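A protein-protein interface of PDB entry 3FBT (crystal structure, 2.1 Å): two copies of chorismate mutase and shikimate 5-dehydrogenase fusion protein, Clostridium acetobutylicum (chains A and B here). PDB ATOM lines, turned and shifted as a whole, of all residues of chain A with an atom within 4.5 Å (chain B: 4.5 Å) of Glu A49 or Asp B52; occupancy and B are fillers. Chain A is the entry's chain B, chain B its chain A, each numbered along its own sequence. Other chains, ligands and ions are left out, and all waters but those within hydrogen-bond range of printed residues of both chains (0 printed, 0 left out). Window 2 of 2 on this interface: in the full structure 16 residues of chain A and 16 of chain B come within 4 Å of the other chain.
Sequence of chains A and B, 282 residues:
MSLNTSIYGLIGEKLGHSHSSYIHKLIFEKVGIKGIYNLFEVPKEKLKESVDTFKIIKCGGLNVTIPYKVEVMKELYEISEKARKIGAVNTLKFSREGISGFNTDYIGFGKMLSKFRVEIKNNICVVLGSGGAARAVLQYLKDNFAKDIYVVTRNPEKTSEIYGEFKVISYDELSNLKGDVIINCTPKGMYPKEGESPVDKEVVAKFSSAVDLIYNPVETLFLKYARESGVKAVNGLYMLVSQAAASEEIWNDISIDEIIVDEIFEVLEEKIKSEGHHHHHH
The side-chain hydroxyl of Thr A53 is in hydrogen-bond range of the side-chain hydroxyl of Thr B53, 2.5 Å away.
The side-chain hydroxyl of Thr B53 is in hydrogen-bond range of the backbone carbonyl oxygen of Glu B49, 3.4 Å away.
The backbone carbonyl oxygen of Lys A46 is in hydrogen-bond range of the side-chain hydroxyl of Ser A50.
The backbone carbonyl oxygen (O) of Glu A49 is in hydrogen-bond range of the side-chain hydroxyl (OG1) of Thr A53 (3.3 Å).
Among the printed residues, merely in contact across the chains: Lys A46 with Ile B56 (3.6 Å), Glu A49 with Glu B49 (3.5 Å), Glu A49 with Asp B52 (3.2 Å), Glu A49 with Thr B53 (3.7 Å), Ser A50 with Thr B53 (3.8 Å), Thr A53 with Glu B49 (3.7 Å) and Thr A53 with Ser B50 (3.8 Å).
Of the printed residues of chain B, Lys A46 touches Ile B56 (3.6 Å).
Of the printed residues of chain B, Glu A49 touches Glu B49, Asp B52 and Thr B53.
Printed residues of chain A within 4 Å of Glu B49: Glu A49 and Thr A53.
Of the printed residues of chain A, Ser B50 touches Thr A53.
Printed residues of chain A within 4 Å of Asp B52: Glu A49 (3.2 Å).
Printed residues of chain A within 4 Å of Thr B53: Glu A49, Ser A50 and Thr A53.
Printed residues of chain A within 4 Å of Ile B56: Lys A46.
The nearest printed residue of chain A that does not touch Asp B52 is Lys A46 (5.7 Å).
Hydrophobic or aromatic side chains of chain B that line the printed part of chain A: Ile B56.
Among the printed residues, no Asp or Glu carboxylate lies within 4 Å of a Lys or Arg side-chain nitrogen of the other chain.
Glu B49 touches its own counterpart, Glu A49.
Glu A49 touches Asp B52, but with the chains exchanged Asp A52 does not touch Glu B49 (6.8 Å).
Glu A49 touches Thr B53, and with the chains exchanged Thr A53 touches Glu B49.
Thr B53 touches its own counterpart, Thr A53.
Of the 8 pairs that touch across the chains among the printed residues, 6 have their exchanged pair printed and touching as well.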
ATOM      1  N   LYS A  46      22.698  18.264 -25.229  1.00  0.00           N
ATOM      2  CA  LYS A  46      21.839  18.939 -24.266  1.00  0.00           C
ATOM      3  C   LYS A  46      22.305  18.842 -22.805  1.00  0.00           C
ATOM      4  O   LYS A  46      21.527  19.089 -21.892  1.00  0.00           O
ATOM      5  CB  LYS A  46      20.442  18.382 -24.392  1.00  0.00           C
ATOM      6  CG  LYS A  46      19.765  18.906 -25.616  1.00  0.00           C
ATOM      7  CD  LYS A  46      19.967  20.443 -25.672  1.00  0.00           C
ATOM      8  CE  LYS A  46      19.388  21.031 -26.960  1.00  0.00           C
ATOM      9  NZ  LYS A  46      18.281  20.166 -27.473  1.00  0.00           N
ATOM     10  N   LEU A  47      23.574  18.495 -22.582  1.00  0.00           N
ATOM     11  CA  LEU A  47      24.001  18.259 -21.207  1.00  0.00           C
ATOM     12  C   LEU A  47      23.970  19.584 -20.452  1.00  0.00           C
ATOM     13  O   LEU A  47      23.297  19.702 -19.435  1.00  0.00           O
ATOM     14  CB  LEU A  47      25.361  17.586 -21.135  1.00  0.00           C
ATOM     15  CG  LEU A  47      25.920  17.164 -19.749  1.00  0.00           C
ATOM     16  CD1 LEU A  47      25.067  16.098 -19.054  1.00  0.00           C
ATOM     17  CD2 LEU A  47      27.284  16.618 -19.950  1.00  0.00           C
ATOM     18  N   LYS A  48      24.704  20.565 -20.957  1.00  0.00           N
ATOM     19  CA  LYS A  48      24.726  21.877 -20.362  1.00  0.00           C
ATOM     20  C   LYS A  48      23.299  22.379 -20.090  1.00  0.00           C
ATOM     21  O   LYS A  48      22.994  22.793 -18.977  1.00  0.00           O
ATOM     22  CB  LYS A  48      25.491  22.885 -21.222  1.00  0.00           C
ATOM     23  CG  LYS A  48      25.902  24.158 -20.505  1.00  0.00           C
ATOM     24  CD  LYS A  48      25.088  25.401 -20.960  1.00  0.00           C
ATOM     25  CE  LYS A  48      24.932  25.439 -22.524  1.00  0.00           C
ATOM     26  NZ  LYS A  48      24.165  26.626 -23.061  1.00  0.00           N
ATOM     27  N   GLU A  49      22.433  22.336 -21.094  1.00  0.00           N
ATOM     28  CA  GLU A  49      21.134  22.915 -20.906  1.00  0.00           C
ATOM     29  C   GLU A  49      20.413  22.160 -19.796  1.00  0.00           C
ATOM     30  O   GLU A  49      19.859  22.770 -18.871  1.00  0.00           O
ATOM     31  CB  GLU A  49      20.319  22.953 -22.207  1.00  0.00           C
ATOM     32  CG  GLU A  49      19.192  24.030 -22.159  1.00  0.00           C
ATOM     33  CD  GLU A  49      18.247  23.945 -23.342  1.00  0.00           C
ATOM     34  OE1 GLU A  49      17.481  22.964 -23.438  1.00  0.00           O
ATOM     35  OE2 GLU A  49      18.283  24.854 -24.199  1.00  0.00           O
ATOM     36  N   SER A  50      20.444  20.835 -19.868  1.00  0.00           N
ATOM     37  CA  SER A  50      19.740  20.041 -18.881  1.00  0.00           C
ATOM     38  C   SER A  50      20.197  20.415 -17.467  1.00  0.00           C
ATOM     39  O   SER A  50      19.365  20.839 -16.671  1.00  0.00           O
ATOM     40  CB  SER A  50      19.930  18.543 -19.100  1.00  0.00           C
ATOM     41  OG  SER A  50      19.210  18.122 -20.243  1.00  0.00           O
ATOM     42  N   VAL A  51      21.482  20.258 -17.154  1.00  0.00           N
ATOM     43  CA  VAL A  51      21.925  20.618 -15.793  1.00  0.00           C
ATOM     44  C   VAL A  51      21.632  22.062 -15.450  1.00  0.00           C
ATOM     45  O   VAL A  51      21.224  22.347 -14.353  1.00  0.00           O
ATOM     46  CB  VAL A  51      23.437  20.249 -15.409  1.00  0.00           C
ATOM     47  CG1 VAL A  51      23.727  18.799 -15.685  1.00  0.00           C
ATOM     48  CG2 VAL A  51      24.376  21.064 -16.133  1.00  0.00           C
ATOM     49  N   ASP A  52      21.815  22.990 -16.373  1.00  0.00           N
ATOM     50  CA  ASP A  52      21.399  24.350 -16.028  1.00  0.00           C
ATOM     51  C   ASP A  52      19.925  24.365 -15.631  1.00  0.00           C
ATOM     52  O   ASP A  52      19.596  24.987 -14.650  1.00  0.00           O
ATOM     53  CB  ASP A  52      21.675  25.341 -17.160  1.00  0.00           C
ATOM     54  CG  ASP A  52      23.195  25.550 -17.406  1.00  0.00           C
ATOM     55  OD1 ASP A  52      23.985  25.411 -16.431  1.00  0.00           O
ATOM     56  OD2 ASP A  52      23.607  25.827 -18.569  1.00  0.00           O
ATOM     57  N   THR A  53      19.031  23.664 -16.354  1.00  0.00           N
ATOM     58  CA  THR A  53      17.604  23.647 -15.912  1.00  0.00           C
ATOM     59  C   THR A  53      17.433  23.022 -14.523  1.00  0.00           C
ATOM     60  O   THR A  53      16.709  23.547 -13.631  1.00  0.00           O
ATOM     61  CB  THR A  53      16.598  22.965 -16.884  1.00  0.00           C
ATOM     62  OG1 THR A  53      16.726  23.499 -18.208  1.00  0.00           O
ATOM     63  CG2 THR A  53      15.105  23.232 -16.398  1.00  0.00           C
ATOM     64  N   LYS B  48      12.768  29.574 -22.463  1.00  0.00           N
ATOM     65  CA  LYS B  48      12.827  28.696 -23.595  1.00  0.00           C
ATOM     66  C   LYS B  48      13.683  27.497 -23.271  1.00  0.00           C
ATOM     67  O   LYS B  48      13.257  26.368 -23.471  1.00  0.00           O
ATOM     68  CB  LYS B  48      13.345  29.405 -24.846  1.00  0.00           C
ATOM     69  CG  LYS B  48      12.856  28.612 -26.046  1.00  0.00           C
ATOM     70  CD  LYS B  48      13.966  27.940 -26.763  1.00  0.00           C
ATOM     71  CE  LYS B  48      14.392  28.865 -27.886  1.00  0.00           C
ATOM     72  NZ  LYS B  48      15.871  29.003 -27.876  1.00  0.00           N
ATOM     73  N   GLU B  49      14.875  27.744 -22.733  1.00  0.00           N
ATOM     74  CA  GLU B  49      15.707  26.634 -22.276  1.00  0.00           C
ATOM     75  C   GLU B  49      15.020  25.696 -21.228  1.00  0.00           C
ATOM     76  O   GLU B  49      15.098  24.479 -21.344  1.00  0.00           O
ATOM     77  CB  GLU B  49      17.081  27.124 -21.781  1.00  0.00           C
ATOM     78  CG  GLU B  49      17.769  28.141 -22.685  1.00  0.00           C
ATOM     79  CD  GLU B  49      17.462  29.568 -22.229  1.00  0.00           C
ATOM     80  OE1 GLU B  49      16.414  30.193 -22.625  1.00  0.00           O
ATOM     81  OE2 GLU B  49      18.301  30.073 -21.440  1.00  0.00           O
ATOM     82  N   SER B  50      14.289  26.226 -20.243  1.00  0.00           N
ATOM     83  CA  SER B  50      13.602  25.303 -19.316  1.00  0.00           C
ATOM     84  C   SER B  50      12.544  24.445 -19.970  1.00  0.00           C
ATOM     85  O   SER B  50      12.433  23.238 -19.711  1.00  0.00           O
ATOM     86  CB  SER B  50      12.958  26.049 -18.138  1.00  0.00           C
ATOM     87  OG  SER B  50      13.728  27.171 -17.882  1.00  0.00           O
ATOM     88  N   VAL B  51      11.671  25.062 -20.748  1.00  0.00           N
ATOM     89  CA  VAL B  51      10.681  24.305 -21.480  1.00  0.00           C
ATOM     90  C   VAL B  51      11.400  23.182 -22.335  1.00  0.00           C
ATOM     91  O   VAL B  51      10.928  22.057 -22.383  1.00  0.00           O
ATOM     92  CB  VAL B  51       9.809  25.317 -22.363  1.00  0.00           C
ATOM     93  CG1 VAL B  51       9.084  24.669 -23.472  1.00  0.00           C
ATOM     94  CG2 VAL B  51       8.799  26.116 -21.457  1.00  0.00           C
ATOM     95  N   ASP B  52      12.533  23.476 -22.982  1.00  0.00           N
ATOM     96  CA  ASP B  52      13.238  22.479 -23.797  1.00  0.00           C
ATOM     97  C   ASP B  52      13.644  21.312 -22.878  1.00  0.00           C
ATOM     98  O   ASP B  52      13.513  20.125 -23.217  1.00  0.00           O
ATOM     99  CB  ASP B  52      14.493  23.080 -24.456  1.00  0.00           C
ATOM    100  CG  ASP B  52      14.187  24.037 -25.648  1.00  0.00           C
ATOM    101  OD1 ASP B  52      13.056  24.039 -26.196  1.00  0.00           O
ATOM    102  OD2 ASP B  52      15.111  24.795 -26.059  1.00  0.00           O
ATOM    103  N   THR B  53      14.151  21.641 -21.697  1.00  0.00           N
ATOM    104  CA  THR B  53      14.526  20.541 -20.802  1.00  0.00           C
ATOM    105  C   THR B  53      13.308  19.768 -20.368  1.00  0.00           C
ATOM    106  O   THR B  53      13.333  18.540 -20.300  1.00  0.00           O
ATOM    107  CB  THR B  53      15.253  21.022 -19.548  1.00  0.00           C
ATOM    108  OG1 THR B  53      16.441  21.718 -19.938  1.00  0.00           O
ATOM    109  CG2 THR B  53      15.572  19.849 -18.702  1.00  0.00           C
ATOM    110  N   PHE B  54      12.209  20.456 -20.087  1.00  0.00           N
ATOM    111  CA  PHE B  54      11.021  19.681 -19.699  1.00  0.00           C
ATOM    112  C   PHE B  54      10.657  18.697 -20.803  1.00  0.00           C
ATOM    113  O   PHE B  54      10.254  17.548 -20.588  1.00  0.00           O
ATOM    114  CB  PHE B  54       9.829  20.606 -19.377  1.00  0.00           C
ATOM    115  CG  PHE B  54       9.928  21.245 -18.001  1.00  0.00           C
ATOM    116  CD1 PHE B  54       9.851  20.464 -16.870  1.00  0.00           C
ATOM    117  CD2 PHE B  54      10.115  22.618 -17.855  1.00  0.00           C
ATOM    118  CE1 PHE B  54       9.974  21.049 -15.598  1.00  0.00           C
ATOM    119  CE2 PHE B  54      10.259  23.198 -16.589  1.00  0.00           C
ATOM    120  CZ  PHE B  54      10.180  22.410 -15.455  1.00  0.00           C
ATOM    121  N   LYS B  55      10.784  19.142 -22.028  1.00  0.00           N
ATOM    122  CA  LYS B  55      10.406  18.244 -23.087  1.00  0.00           C
ATOM    123  C   LYS B  55      11.413  17.040 -23.058  1.00  0.00           C
ATOM    124  O   LYS B  55      11.025  15.877 -23.155  1.00  0.00           O
ATOM    125  CB  LYS B  55      10.441  19.030 -24.404  1.00  0.00           C
ATOM    126  CG  LYS B  55       9.527  18.472 -25.479  1.00  0.00           C
ATOM    127  CD  LYS B  55       9.392  19.458 -26.680  1.00  0.00           C
ATOM    128  CE  LYS B  55      10.637  20.314 -26.870  1.00  0.00           C
ATOM    129  NZ  LYS B  55      10.481  21.270 -28.036  1.00  0.00           N
ATOM    130  N   ILE B  56      12.681  17.341 -22.834  1.00  0.00           N
ATOM    131  CA  ILE B  56      13.736  16.293 -22.742  1.00  0.00           C
ATOM    132  C   ILE B  56      13.594  15.294 -21.596  1.00  0.00           C
ATOM    133  O   ILE B  56      13.724  14.106 -21.778  1.00  0.00           O
ATOM    134  CB  ILE B  56      15.140  16.883 -22.793  1.00  0.00           C
ATOM    135  CG1 ILE B  56      15.400  17.517 -24.177  1.00  0.00           C
ATOM    136  CG2 ILE B  56      16.152  15.795 -22.580  1.00  0.00           C
ATOM    137  CD1 ILE B  56      16.525  18.563 -24.134  1.00  0.00           C
